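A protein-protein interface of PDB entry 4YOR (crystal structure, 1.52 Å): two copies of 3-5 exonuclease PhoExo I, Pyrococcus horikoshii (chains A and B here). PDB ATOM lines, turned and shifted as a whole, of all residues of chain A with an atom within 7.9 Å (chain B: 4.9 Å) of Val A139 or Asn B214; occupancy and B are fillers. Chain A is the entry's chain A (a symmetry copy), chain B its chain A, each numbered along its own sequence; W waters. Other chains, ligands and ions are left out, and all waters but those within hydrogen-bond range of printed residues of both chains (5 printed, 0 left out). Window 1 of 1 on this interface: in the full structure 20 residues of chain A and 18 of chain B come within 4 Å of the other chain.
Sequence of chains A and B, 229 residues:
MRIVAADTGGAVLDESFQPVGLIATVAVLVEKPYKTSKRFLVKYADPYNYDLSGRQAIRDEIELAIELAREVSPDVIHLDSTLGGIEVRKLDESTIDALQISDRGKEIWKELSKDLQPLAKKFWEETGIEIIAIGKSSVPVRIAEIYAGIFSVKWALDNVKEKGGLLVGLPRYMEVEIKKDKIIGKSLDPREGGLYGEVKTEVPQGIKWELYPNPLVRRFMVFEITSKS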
ATOM      1  N   MET A   1     -23.338 -13.459 -21.441  1.00  0.00           N
ATOM      2  CA  MET A   1     -23.753 -14.140 -22.657  1.00  0.00           C
ATOM      3  C   MET A   1     -23.542 -15.640 -22.547  1.00  0.00           C
ATOM      4  O   MET A   1     -22.592 -16.104 -21.901  1.00  0.00           O
ATOM      5  CB  MET A   1     -22.975 -13.615 -23.864  1.00  0.00           C
ATOM      6  CG  MET A   1     -23.423 -12.272 -24.411  1.00  0.00           C
ATOM      7  SD  MET A   1     -22.583 -11.991 -25.986  1.00  0.00           S
ATOM      8  CE  MET A   1     -23.242 -13.325 -26.958  1.00  0.00           C
ATOM      9  N   ILE A   3     -23.203 -18.852 -25.179  1.00  0.00           N
ATOM     10  CA  ILE A   3     -22.926 -19.050 -26.595  1.00  0.00           C
ATOM     11  C   ILE A   3     -22.687 -20.520 -26.906  1.00  0.00           C
ATOM     12  O   ILE A   3     -21.926 -21.186 -26.198  1.00  0.00           O
ATOM     13  CB  ILE A   3     -21.687 -18.232 -27.021  1.00  0.00           C
ATOM     14  CG1 ILE A   3     -21.913 -16.747 -26.741  1.00  0.00           C
ATOM     15  CG2 ILE A   3     -21.373 -18.460 -28.490  1.00  0.00           C
ATOM     16  CD1 ILE A   3     -20.621 -15.911 -26.736  1.00  0.00           C
ATOM     17  N   ALA A   5     -21.047 -22.878 -29.859  1.00  0.00           N
ATOM     18  CA  ALA A   5     -20.208 -22.813 -31.049  1.00  0.00           C
ATOM     19  C   ALA A   5     -19.780 -24.203 -31.458  1.00  0.00           C
ATOM     20  O   ALA A   5     -19.894 -25.138 -30.676  1.00  0.00           O
ATOM     21  CB  ALA A   5     -18.980 -21.928 -30.802  1.00  0.00           C
ATOM     22  N   VAL A  28     -19.836 -26.759 -28.368  1.00  0.00           N
ATOM     23  CA  VAL A  28     -19.639 -26.377 -26.964  1.00  0.00           C
ATOM     24  C   VAL A  28     -20.636 -25.325 -26.540  1.00  0.00           C
ATOM     25  O   VAL A  28     -21.058 -24.501 -27.354  1.00  0.00           O
ATOM     26  CB  VAL A  28     -18.220 -25.803 -26.695  1.00  0.00           C
ATOM     27  CG1 VAL A  28     -17.158 -26.871 -26.866  1.00  0.00           C
ATOM     28  CG2 VAL A  28     -17.905 -24.591 -27.597  1.00  0.00           C
ATOM     29  N   VAL A  30     -20.485 -22.156 -24.023  1.00  0.00           N
ATOM     30  CA  VAL A  30     -19.487 -21.340 -23.335  1.00  0.00           C
ATOM     31  C   VAL A  30     -20.183 -20.190 -22.624  1.00  0.00           C
ATOM     32  O   VAL A  30     -21.057 -19.527 -23.201  1.00  0.00           O
ATOM     33  CB  VAL A  30     -18.435 -20.812 -24.311  1.00  0.00           C
ATOM     34  CG1 VAL A  30     -17.426 -19.932 -23.588  1.00  0.00           C
ATOM     35  CG2 VAL A  30     -17.700 -21.984 -24.986  1.00  0.00           C
ATOM     36  N   PRO A  33     -16.329 -17.176 -17.420  1.00  0.00           N
ATOM     37  CA  PRO A  33     -15.435 -16.174 -18.033  1.00  0.00           C
ATOM     38  C   PRO A  33     -14.885 -16.508 -19.432  1.00  0.00           C
ATOM     39  O   PRO A  33     -13.846 -15.955 -19.820  1.00  0.00           O
ATOM     40  CB  PRO A  33     -14.297 -16.094 -17.015  1.00  0.00           C
ATOM     41  CG  PRO A  33     -14.178 -17.513 -16.537  1.00  0.00           C
ATOM     42  CD  PRO A  33     -15.617 -17.969 -16.395  1.00  0.00           C
ATOM     43  N   TYR A  34     -15.567 -17.381 -20.171  1.00  0.00           N
ATOM     44  CA  TYR A  34     -15.276 -17.634 -21.586  1.00  0.00           C
ATOM     45  C   TYR A  34     -13.876 -18.191 -21.820  1.00  0.00           C
ATOM     46  O   TYR A  34     -13.227 -17.844 -22.811  1.00  0.00           O
ATOM     47  CB  TYR A  34     -15.489 -16.340 -22.412  1.00  0.00           C
ATOM     48  CG  TYR A  34     -16.779 -15.621 -22.061  1.00  0.00           C
ATOM     49  CD1 TYR A  34     -18.018 -16.129 -22.460  1.00  0.00           C
ATOM     50  CD2 TYR A  34     -16.765 -14.461 -21.298  1.00  0.00           C
ATOM     51  CE1 TYR A  34     -19.198 -15.485 -22.115  1.00  0.00           C
ATOM     52  CE2 TYR A  34     -17.948 -13.813 -20.947  1.00  0.00           C
ATOM     53  CZ  TYR A  34     -19.155 -14.330 -21.362  1.00  0.00           C
ATOM     54  OH  TYR A  34     -20.318 -13.666 -21.004  1.00  0.00           O
ATOM     55  N   LYS A  35     -13.415 -19.051 -20.911  1.00  0.00           N
ATOM     56  CA  LYS A  35     -12.101 -19.700 -21.068  1.00  0.00           C
ATOM     57  C   LYS A  35     -12.197 -21.187 -21.407  1.00  0.00           C
ATOM     58  O   LYS A  35     -11.280 -21.747 -22.001  1.00  0.00           O
ATOM     59  CB  LYS A  35     -11.270 -19.536 -19.799  1.00  0.00           C
ATOM     60  CG  LYS A  35     -10.904 -18.083 -19.497  1.00  0.00           C
ATOM     61  CD  LYS A  35     -10.129 -17.972 -18.184  1.00  0.00           C
ATOM     62  CE  LYS A  35      -9.753 -16.533 -17.869  1.00  0.00           C
ATOM     63  NZ  LYS A  35      -9.039 -16.436 -16.554  1.00  0.00           N
ATOM     64  N   THR A  36     -13.289 -21.833 -21.006  1.00  0.00           N
ATOM     65  CA  THR A  36     -13.462 -23.262 -21.286  1.00  0.00           C
ATOM     66  C   THR A  36     -14.934 -23.576 -21.520  1.00  0.00           C
ATOM     67  O   THR A  36     -15.779 -22.664 -21.588  1.00  0.00           O
ATOM     68  CB  THR A  36     -12.889 -24.126 -20.121  1.00  0.00           C
ATOM     69  OG1 THR A  36     -12.780 -25.505 -20.528  1.00  0.00           O
ATOM     70  CG2 THR A  36     -13.745 -24.009 -18.847  1.00  0.00           C
ATOM     71  N   HIS A  78     -22.365 -19.470 -32.671  1.00  0.00           N
ATOM     72  CA  HIS A  78     -21.212 -19.076 -33.490  1.00  0.00           C
ATOM     73  C   HIS A  78     -20.772 -20.201 -34.420  1.00  0.00           C
ATOM     74  O   HIS A  78     -20.414 -21.287 -33.964  1.00  0.00           O
ATOM     75  CB  HIS A  78     -20.034 -18.683 -32.596  1.00  0.00           C
ATOM     76  CG  HIS A  78     -20.221 -17.390 -31.875  1.00  0.00           C
ATOM     77  ND1 HIS A  78     -19.228 -16.828 -31.101  1.00  0.00           N
ATOM     78  CD2 HIS A  78     -21.266 -16.528 -31.830  1.00  0.00           C
ATOM     79  CE1 HIS A  78     -19.654 -15.683 -30.602  1.00  0.00           C
ATOM     80  NE2 HIS A  78     -20.888 -15.475 -31.035  1.00  0.00           N
ATOM     81  N   ILE A 134     -19.098 -16.000 -37.745  1.00  0.00           N
ATOM     82  CA  ILE A 134     -18.125 -15.163 -37.065  1.00  0.00           C
ATOM     83  C   ILE A 134     -16.708 -15.732 -37.195  1.00  0.00           C
ATOM     84  O   ILE A 134     -15.740 -14.988 -37.278  1.00  0.00           O
ATOM     85  CB  ILE A 134     -18.524 -14.976 -35.570  1.00  0.00           C
ATOM     86  CG1 ILE A 134     -17.471 -14.165 -34.816  1.00  0.00           C
ATOM     87  CG2 ILE A 134     -18.789 -16.328 -34.897  1.00  0.00           C
ATOM     88  CD1 ILE A 134     -17.981 -13.594 -33.490  1.00  0.00           C
ATOM     89  N   GLY A 135     -16.581 -17.056 -37.230  1.00  0.00           N
ATOM     90  CA  GLY A 135     -15.286 -17.655 -37.506  1.00  0.00           C
ATOM     91  C   GLY A 135     -14.171 -17.344 -36.520  1.00  0.00           C
ATOM     92  O   GLY A 135     -14.338 -17.491 -35.296  1.00  0.00           O
ATOM     93  N   LYS A 136     -13.036 -16.911 -37.055  1.00  0.00           N
ATOM     94  CA  LYS A 136     -11.825 -16.737 -36.261  1.00  0.00           C
ATOM     95  C   LYS A 136     -11.936 -15.645 -35.188  1.00  0.00           C
ATOM     96  O   LYS A 136     -11.091 -15.566 -34.306  1.00  0.00           O
ATOM     97  CB  LYS A 136     -10.640 -16.448 -37.185  1.00  0.00           C
ATOM     98  CG  LYS A 136     -10.379 -17.554 -38.204  1.00  0.00           C
ATOM     99  CD  LYS A 136     -10.468 -18.946 -37.578  1.00  0.00           C
ATOM    100  CE  LYS A 136     -10.064 -20.035 -38.573  1.00  0.00           C
ATOM    101  NZ  LYS A 136     -10.699 -21.353 -38.271  1.00  0.00           N
ATOM    102  N   SER A 137     -12.976 -14.823 -35.244  1.00  0.00           N
ATOM    103  CA  SER A 137     -13.155 -13.795 -34.221  1.00  0.00           C
ATOM    104  C   SER A 137     -13.728 -14.373 -32.917  1.00  0.00           C
ATOM    105  O   SER A 137     -13.631 -13.742 -31.859  1.00  0.00           O
ATOM    106  CB  SER A 137     -14.065 -12.678 -34.741  1.00  0.00           C
ATOM    107  OG  SER A 137     -14.040 -11.558 -33.871  1.00  0.00           O
ATOM    108  N   SER A 138     -14.313 -15.565 -32.995  1.00  0.00           N
ATOM    109  CA  SER A 138     -15.067 -16.131 -31.873  1.00  0.00           C
ATOM    110  C   SER A 138     -14.185 -16.901 -30.891  1.00  0.00           C
ATOM    111  O   SER A 138     -13.502 -17.847 -31.295  1.00  0.00           O
ATOM    112  CB  SER A 138     -16.147 -17.071 -32.411  1.00  0.00           C
ATOM    113  OG  SER A 138     -16.739 -17.829 -31.368  1.00  0.00           O
ATOM    114  N   VAL A 139     -14.271 -16.570 -29.601  1.00  0.00           N
ATOM    115  CA  VAL A 139     -13.603 -17.403 -28.600  1.00  0.00           C
ATOM    116  C   VAL A 139     -14.324 -18.764 -28.425  1.00  0.00           C
ATOM    117  O   VAL A 139     -13.650 -19.798 -28.350  1.00  0.00           O
ATOM    118  CB  VAL A 139     -13.473 -16.649 -27.255  1.00  0.00           C
ATOM    119  CG1 VAL A 139     -12.948 -17.566 -26.143  1.00  0.00           C
ATOM    120  CG2 VAL A 139     -12.533 -15.440 -27.447  1.00  0.00           C
ATOM    121  N   PRO A 140     -15.672 -18.780 -28.371  1.00  0.00           N
ATOM    122  CA  PRO A 140     -16.302 -20.106 -28.275  1.00  0.00           C
ATOM    123  C   PRO A 140     -15.933 -21.030 -29.445  1.00  0.00           C
ATOM    124  O   PRO A 140     -15.773 -22.224 -29.193  1.00  0.00           O
ATOM    125  CB  PRO A 140     -17.799 -19.772 -28.241  1.00  0.00           C
ATOM    126  CG  PRO A 140     -17.836 -18.427 -27.513  1.00  0.00           C
ATOM    127  CD  PRO A 140     -16.640 -17.697 -28.105  1.00  0.00           C
ATOM    128  N   VAL A 141     -15.782 -20.521 -30.669  1.00  0.00           N
ATOM    129  CA  VAL A 141     -15.335 -21.385 -31.772  1.00  0.00           C
ATOM    130  C   VAL A 141     -13.949 -21.970 -31.459  1.00  0.00           C
ATOM    131  O   VAL A 141     -13.715 -23.159 -31.659  1.00  0.00           O
ATOM    132  CB  VAL A 141     -15.313 -20.631 -33.134  1.00  0.00           C
ATOM    133  CG1 VAL A 141     -14.543 -21.435 -34.203  1.00  0.00           C
ATOM    134  CG2 VAL A 141     -16.739 -20.335 -33.617  1.00  0.00           C
ATOM    135  N   ARG A 142     -13.031 -21.155 -30.950  1.00  0.00           N
ATOM    136  CA  ARG A 142     -11.696 -21.639 -30.588  1.00  0.00           C
ATOM    137  C   ARG A 142     -11.738 -22.683 -29.462  1.00  0.00           C
ATOM    138  O   ARG A 142     -10.988 -23.663 -29.483  1.00  0.00           O
ATOM    139  CB  ARG A 142     -10.806 -20.453 -30.193  1.00  0.00           C
ATOM    140  CG  ARG A 142      -9.434 -20.842 -29.650  1.00  0.00           C
ATOM    141  CD  ARG A 142      -8.585 -21.628 -30.653  1.00  0.00           C
ATOM    142  NE  ARG A 142      -7.231 -21.739 -30.127  1.00  0.00           N
ATOM    143  CZ  ARG A 142      -6.304 -22.577 -30.574  1.00  0.00           C
ATOM    144  NH1 ARG A 142      -6.576 -23.435 -31.558  1.00  0.00           N
ATOM    145  NH2 ARG A 142      -5.106 -22.568 -29.998  1.00  0.00           N
ATOM    146  N   ILE A 143     -12.618 -22.485 -28.481  1.00  0.00           N
ATOM    147  CA  ILE A 143     -12.776 -23.474 -27.420  1.00  0.00           C
ATOM    148  C   ILE A 143     -13.313 -24.799 -28.001  1.00  0.00           C
ATOM    149  O   ILE A 143     -12.829 -25.876 -27.631  1.00  0.00           O
ATOM    150  CB  ILE A 143     -13.691 -22.933 -26.297  1.00  0.00           C
ATOM    151  CG1 ILE A 143     -12.963 -21.808 -25.551  1.00  0.00           C
ATOM    152  CG2 ILE A 143     -14.103 -24.051 -25.319  1.00  0.00           C
ATOM    153  CD1 ILE A 143     -13.882 -20.946 -24.666  1.00  0.00           C
ATOM    154  N   ALA A 144     -14.271 -24.729 -28.927  1.00  0.00           N
ATOM    155  CA  ALA A 144     -14.725 -25.935 -29.632  1.00  0.00           C
ATOM    156  C   ALA A 144     -13.562 -26.622 -30.326  1.00  0.00           C
ATOM    157  O   ALA A 144     -13.445 -27.857 -30.286  1.00  0.00           O
ATOM    158  CB  ALA A 144     -15.809 -25.590 -30.642  1.00  0.00           C
ATOM    159  N   GLU A 145     -12.708 -25.820 -30.962  1.00  0.00           N
ATOM    160  CA  GLU A 145     -11.557 -26.348 -31.686  1.00  0.00           C
ATOM    161  C   GLU A 145     -10.563 -27.043 -30.749  1.00  0.00           C
ATOM    162  O   GLU A 145     -10.037 -28.127 -31.068  1.00  0.00           O
ATOM    163  CB  GLU A 145     -10.870 -25.219 -32.459  1.00  0.00           C
ATOM    164  CG  GLU A 145      -9.806 -25.779 -33.409  1.00  0.00           C
ATOM    165  CD  GLU A 145      -9.047 -24.721 -34.185  1.00  0.00           C
ATOM    166  OE1 GLU A 145      -8.669 -23.678 -33.604  1.00  0.00           O
ATOM    167  OE2 GLU A 145      -8.820 -24.963 -35.394  1.00  0.00           O
ATOM    168  N   ILE A 146     -10.299 -26.425 -29.601  1.00  0.00           N
ATOM    169  CA  ILE A 146      -9.430 -27.039 -28.601  1.00  0.00           C
ATOM    170  C   ILE A 146     -10.043 -28.377 -28.151  1.00  0.00           C
ATOM    171  O   ILE A 146      -9.331 -29.378 -28.042  1.00  0.00           O
ATOM    172  CB  ILE A 146      -9.210 -26.077 -27.417  1.00  0.00           C
ATOM    173  CG1 ILE A 146      -8.311 -24.923 -27.877  1.00  0.00           C
ATOM    174  CG2 ILE A 146      -8.563 -26.775 -26.217  1.00  0.00           C
ATOM    175  CD1 ILE A 146      -8.297 -23.733 -26.894  1.00  0.00           C
ATOM    176  N   GLU A 192      -4.525 -15.422 -26.237  1.00  0.00           N
ATOM    177  CA  GLU A 192      -5.927 -15.837 -26.162  1.00  0.00           C
ATOM    178  C   GLU A 192      -6.504 -15.812 -24.738  1.00  0.00           C
ATOM    179  O   GLU A 192      -7.722 -15.936 -24.566  1.00  0.00           O
ATOM    180  CB  GLU A 192      -6.105 -17.229 -26.792  1.00  0.00           C
ATOM    181  CG  GLU A 192      -5.920 -17.214 -28.313  1.00  0.00           C
ATOM    182  CD  GLU A 192      -6.264 -18.527 -28.995  1.00  0.00           C
ATOM    183  OE1 GLU A 192      -6.806 -18.484 -30.113  1.00  0.00           O
ATOM    184  OE2 GLU A 192      -5.965 -19.593 -28.441  1.00  0.00           O
ATOM    185  N   GLY A 193      -5.651 -15.619 -23.728  1.00  0.00           N
ATOM    186  CA  GLY A 193      -6.108 -15.337 -22.373  1.00  0.00           C
ATOM    187  C   GLY A 193      -6.381 -16.544 -21.490  1.00  0.00           C
ATOM    188  O   GLY A 193      -7.041 -16.417 -20.455  1.00  0.00           O
ATOM    189  N   LEU A 195      -7.187 -20.169 -22.689  1.00  0.00           N
ATOM    190  CA  LEU A 195      -8.247 -21.066 -23.137  1.00  0.00           C
ATOM    191  C   LEU A 195      -7.832 -22.523 -22.950  1.00  0.00           C
ATOM    192  O   LEU A 195      -6.686 -22.894 -23.231  1.00  0.00           O
ATOM    193  CB  LEU A 195      -8.588 -20.796 -24.602  1.00  0.00           C
ATOM    194  CG  LEU A 195      -8.840 -19.325 -24.951  1.00  0.00           C
ATOM    195  CD1 LEU A 195      -9.237 -19.244 -26.407  1.00  0.00           C
ATOM    196  CD2 LEU A 195      -9.956 -18.768 -24.082  1.00  0.00           C
ATOM    197  N   LEU B  13     -18.284  -1.162 -23.303  1.00  0.00           N
ATOM    198  CA  LEU B  13     -19.107  -2.165 -23.986  1.00  0.00           C
ATOM    199  C   LEU B  13     -20.483  -2.283 -23.355  1.00  0.00           C
ATOM    200  O   LEU B  13     -20.635  -2.042 -22.162  1.00  0.00           O
ATOM    201  CB  LEU B  13     -18.431  -3.541 -23.945  1.00  0.00           C
ATOM    202  CG  LEU B  13     -16.955  -3.646 -24.345  1.00  0.00           C
ATOM    203  CD1 LEU B  13     -16.482  -5.098 -24.226  1.00  0.00           C
ATOM    204  CD2 LEU B  13     -16.761  -3.141 -25.755  1.00  0.00           C
ATOM    205  N   PHE B  17     -21.409  -7.096 -25.248  1.00  0.00           N
ATOM    206  CA  PHE B  17     -20.012  -6.836 -25.630  1.00  0.00           C
ATOM    207  C   PHE B  17     -19.869  -5.966 -26.879  1.00  0.00           C
ATOM    208  O   PHE B  17     -18.821  -5.950 -27.507  1.00  0.00           O
ATOM    209  CB  PHE B  17     -19.239  -8.158 -25.822  1.00  0.00           C
ATOM    210  CG  PHE B  17     -19.155  -8.988 -24.571  1.00  0.00           C
ATOM    211  CD1 PHE B  17     -18.280  -8.643 -23.550  1.00  0.00           C
ATOM    212  CD2 PHE B  17     -19.957 -10.094 -24.405  1.00  0.00           C
ATOM    213  CE1 PHE B  17     -18.224  -9.401 -22.381  1.00  0.00           C
ATOM    214  CE2 PHE B  17     -19.907 -10.858 -23.245  1.00  0.00           C
ATOM    215  CZ  PHE B  17     -19.034 -10.508 -22.234  1.00  0.00           C
ATOM    216  N   TYR B 212     -11.172 -11.055 -18.316  1.00  0.00           N
ATOM    217  CA  TYR B 212     -11.452 -12.314 -19.019  1.00  0.00           C
ATOM    218  C   TYR B 212     -11.579 -12.077 -20.519  1.00  0.00           C
ATOM    219  O   TYR B 212     -11.732 -10.946 -20.957  1.00  0.00           O
ATOM    220  CB  TYR B 212     -12.723 -12.978 -18.464  1.00  0.00           C
ATOM    221  CG  TYR B 212     -13.956 -12.108 -18.487  1.00  0.00           C
ATOM    222  CD1 TYR B 212     -14.676 -11.913 -19.661  1.00  0.00           C
ATOM    223  CD2 TYR B 212     -14.414 -11.495 -17.322  1.00  0.00           C
ATOM    224  CE1 TYR B 212     -15.819 -11.114 -19.680  1.00  0.00           C
ATOM    225  CE2 TYR B 212     -15.554 -10.697 -17.330  1.00  0.00           C
ATOM    226  CZ  TYR B 212     -16.247 -10.510 -18.512  1.00  0.00           C
ATOM    227  OH  TYR B 212     -17.381  -9.728 -18.526  1.00  0.00           O
ATOM    228  N   PRO B 213     -11.513 -13.151 -21.319  1.00  0.00           N
ATOM    229  CA  PRO B 213     -11.645 -12.973 -22.769  1.00  0.00           C
ATOM    230  C   PRO B 213     -12.986 -12.377 -23.220  1.00  0.00           C
ATOM    231  O   PRO B 213     -14.044 -12.794 -22.750  1.00  0.00           O
ATOM    232  CB  PRO B 213     -11.490 -14.404 -23.306  1.00  0.00           C
ATOM    233  CG  PRO B 213     -10.618 -15.092 -22.287  1.00  0.00           C
ATOM    234  CD  PRO B 213     -11.099 -14.522 -20.963  1.00  0.00           C
ATOM    235  N   ASN B 214     -12.917 -11.399 -24.125  1.00  0.00           N
ATOM    236  CA  ASN B 214     -14.089 -10.987 -24.902  1.00  0.00           C
ATOM    237  C   ASN B 214     -14.501 -12.137 -25.824  1.00  0.00           C
ATOM    238  O   ASN B 214     -13.745 -12.470 -26.752  1.00  0.00           O
ATOM    239  CB  ASN B 214     -13.759  -9.726 -25.722  1.00  0.00           C
ATOM    240  CG  ASN B 214     -14.978  -9.159 -26.465  1.00  0.00           C
ATOM    241  OD1 ASN B 214     -15.895  -9.888 -26.843  1.00  0.00           O
ATOM    242  ND2 ASN B 214     -14.974  -7.844 -26.684  1.00  0.00           N
ATOM    243  N   PRO B 215     -15.682 -12.741 -25.598  1.00  0.00           N
ATOM    244  CA  PRO B 215     -15.983 -13.941 -26.398  1.00  0.00           C
ATOM    245  C   PRO B 215     -16.232 -13.629 -27.878  1.00  0.00           C
ATOM    246  O   PRO B 215     -16.202 -14.542 -28.699  1.00  0.00           O
ATOM    247  CB  PRO B 215     -17.242 -14.512 -25.736  1.00  0.00           C
ATOM    248  CG  PRO B 215     -17.906 -13.294 -25.088  1.00  0.00           C
ATOM    249  CD  PRO B 215     -16.749 -12.455 -24.610  1.00  0.00           C
ATOM    250  N   LEU B 216     -16.474 -12.363 -28.208  1.00  0.00           N
ATOM    251  CA  LEU B 216     -16.764 -11.989 -29.595  1.00  0.00           C
ATOM    252  C   LEU B 216     -15.532 -11.514 -30.362  1.00  0.00           C
ATOM    253  O   LEU B 216     -15.603 -11.321 -31.576  1.00  0.00           O
ATOM    254  CB  LEU B 216     -17.815 -10.875 -29.641  1.00  0.00           C
ATOM    255  CG  LEU B 216     -19.078 -11.119 -28.823  1.00  0.00           C
ATOM    256  CD1 LEU B 216     -20.139 -10.077 -29.201  1.00  0.00           C
ATOM    257  CD2 LEU B 216     -19.637 -12.531 -28.966  1.00  0.00           C
ATOM    258  N   VAL B 217     -14.424 -11.274 -29.662  1.00  0.00           N
ATOM    259  CA  VAL B 217     -13.224 -10.744 -30.299  1.00  0.00           C
ATOM    260  C   VAL B 217     -11.982 -11.423 -29.726  1.00  0.00           C
ATOM    261  O   VAL B 217     -11.367 -10.936 -28.770  1.00  0.00           O
ATOM    262  CB  VAL B 217     -13.081  -9.206 -30.127  1.00  0.00           C
ATOM    263  CG1 VAL B 217     -12.023  -8.675 -31.087  1.00  0.00           C
ATOM    264  CG2 VAL B 217     -14.418  -8.466 -30.339  1.00  0.00           C
ATOM    265  N   ARG B 218     -11.615 -12.542 -30.342  1.00  0.00           N
ATOM    266  CA  ARG B 218     -10.489 -13.358 -29.910  1.00  0.00           C
ATOM    267  C   ARG B 218      -9.212 -12.527 -29.751  1.00  0.00           C
ATOM    268  O   ARG B 218      -8.912 -11.666 -30.582  1.00  0.00           O
ATOM    269  CB  ARG B 218     -10.283 -14.514 -30.917  1.00  0.00           C
ATOM    270  CG  ARG B 218      -9.441 -15.694 -30.433  1.00  0.00           C
ATOM    271  CD  ARG B 218      -9.247 -16.776 -31.563  1.00  0.00           C
ATOM    272  NE  ARG B 218     -10.501 -17.366 -32.020  1.00  0.00           N
ATOM    273  CZ  ARG B 218     -10.602 -18.241 -33.025  1.00  0.00           C
ATOM    274  NH1 ARG B 218      -9.509 -18.611 -33.703  1.00  0.00           N
ATOM    275  NH2 ARG B 218     -11.793 -18.738 -33.366  1.00  0.00           N
ATOM    276  N   PHE B 220      -8.721 -10.313 -27.453  1.00  0.00           N
ATOM    277  CA  PHE B 220      -9.006  -9.071 -26.720  1.00  0.00           C
ATOM    278  C   PHE B 220      -9.643  -9.415 -25.376  1.00  0.00           C
ATOM    279  O   PHE B 220     -10.549 -10.249 -25.312  1.00  0.00           O
ATOM    280  CB  PHE B 220      -9.958  -8.149 -27.484  1.00  0.00           C
ATOM    281  CG  PHE B 220      -9.363  -7.496 -28.703  1.00  0.00           C
ATOM    282  CD1 PHE B 220      -9.034  -8.247 -29.825  1.00  0.00           C
ATOM    283  CD2 PHE B 220      -9.196  -6.122 -28.750  1.00  0.00           C
ATOM    284  CE1 PHE B 220      -8.524  -7.639 -30.964  1.00  0.00           C
ATOM    285  CE2 PHE B 220      -8.688  -5.512 -29.884  1.00  0.00           C
ATOM    286  CZ  PHE B 220      -8.357  -6.267 -30.993  1.00  0.00           C
ATOM    287  N   MET B 221      -9.179  -8.773 -24.308  1.00  0.00           N
ATOM    288  CA  MET B 221      -9.731  -9.015 -22.976  1.00  0.00           C
ATOM    289  C   MET B 221     -10.719  -7.937 -22.557  1.00  0.00           C
ATOM    290  O   MET B 221     -10.696  -6.820 -23.086  1.00  0.00           O
ATOM    291  CB  MET B 221      -8.611  -9.102 -21.936  1.00  0.00           C
ATOM    292  CG  MET B 221      -7.481 -10.076 -22.290  1.00  0.00           C
ATOM    293  SD  MET B 221      -8.080 -11.770 -22.403  1.00  0.00           S
ATOM    294  CE  MET B 221      -7.659 -12.165 -24.095  1.00  0.00           C
ATOM    295  N   VAL B 222     -11.588  -8.295 -21.618  1.00  0.00           N
ATOM    296  CA  VAL B 222     -12.534  -7.364 -21.012  1.00  0.00           C
ATOM    297  C   VAL B 222     -12.158  -7.145 -19.552  1.00  0.00           C
ATOM    298  O   VAL B 222     -11.843  -8.097 -18.832  1.00  0.00           O
ATOM    299  CB  VAL B 222     -13.983  -7.909 -21.105  1.00  0.00           C
ATOM    300  CG1 VAL B 222     -14.978  -7.017 -20.342  1.00  0.00           C
ATOM    301  CG2 VAL B 222     -14.397  -8.066 -22.563  1.00  0.00           C
HETATM  302  O   HOH W   1     -20.212 -11.576 -18.984  1.00  0.00           O
HETATM  303  O   HOH W   2      -8.105 -15.651 -34.731  1.00  0.00           O
HETATM  304  O   HOH W   3      -8.146 -21.327 -34.541  1.00  0.00           O
HETATM  305  O   HOH W   4     -11.132 -21.998 -34.179  1.00  0.00           O
HETATM  306  O   HOH W   5      -6.844 -19.151 -32.749  1.00  0.00           O
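The backbone NH (N) of Val B217 is in hydrogen-bond range of the backbone carbonyl oxygen (O) of Ser A137, 3.4 Å away.
The backbone NH (N) of Arg B218 is in hydrogen-bond range of the backbone carbonyl oxygen (O) of Ser A137 (2.8 Å).
The guanidinium group (NE) of Arg B218 sits at hydrogen-bond distance from the backbone carbonyl oxygen (O) of Lys A136, at 3.0 Å.
The backbone carbonyl oxygen of Pro B215 sits at hydrogen-bond distance from the backbone NH of Val A139 (2.9 Å).
O of Leu B216 lies within hydrogen-bond range of OG of Ser A137.
The guanidinium group (NH2) of Arg B218 sits at hydrogen-bond distance from the backbone carbonyl oxygen (O) of Gly A135 (3.4 Å).
O of Ser A138 is in hydrogen-bond range of NH2 of Arg B218 (2.8 Å).
Hydrophobic or aromatic side chains of chain B that line the printed part of chain A: Phe B17, Tyr B212, Pro B213, Pro B215, Leu B216 and Met B221.
Val A139 touches just these residues of chain B: Asn B214, Pro B215 and Arg B218.
Asn B214 touches just one residue of chain A: Val A139 (3.3 Å).
Of the printed residues of chain B, Gly A193 touches Met B221.
Of the printed residues of chain B, Tyr A34 touches Phe B17, Tyr B212, Pro B213 and Pro B215.
Printed residues of chain A within 4 Å of Phe B17: Met A1 and Tyr A34.
Val A30 touches none of the printed residues of chain B.
The nearest residue of chain A that does not touch Asn B214 is Ser A137 (5.3 Å).
Among the printed residues, pairs that only touch across the chains: Pro A140 with Pro B215, Val A139 with Asn B214, Pro A33 with Pro B213, Glu A192 with Arg B218, Pro A33 with Tyr B212, Tyr A34 with Pro B213, His A78 with Leu B216, Arg A142 with Arg B218, Met A1 with Phe B17, Tyr A34 with Phe B17, Tyr A34 with Tyr B212, Ser A138 with Pro B215, Tyr A34 with Pro B215, Glu A192 with Pro B213, Ile A3 with Pro B215, Glu A192 with Met B221, Ile A134 with Leu B216, Val A139 with Arg B218, Lys A35 with Pro B213, Gly A193 with Met B221 and Val A141 with Arg B218.
Water W5 lies within hydrogen-bond range of OE1 of Glu A192 (2.7 Å) and NH1 of Arg B218 (2.9 Å).
Water W1 lies within hydrogen-bond range of the side-chain hydroxyl (OH) of Tyr A34 (2.9 Å) and the side-chain hydroxyl (OH) of Tyr B212 (3.4 Å).
Water W2 bridges O of Lys A136 (3.0 Å) and NH1 of Arg B218 (3.4 Å).
The side-chain carboxylate of Glu A192 lies within salt-bridge range of the guanidinium group of Arg A142, 3.0 Å away.
N of Val A30 lies within hydrogen-bond range of O of Ile A3, at 2.8 Å.
The backbone carbonyl oxygen (O) of Tyr B212 lies within hydrogen-bond range of the backbone NH (N) of Val B222, 2.7 Å away.
No position is printed for both chains.
Of the 28 pairs that touch across the chains among the printed residues, none has its exchanged pair printed and touching as well.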
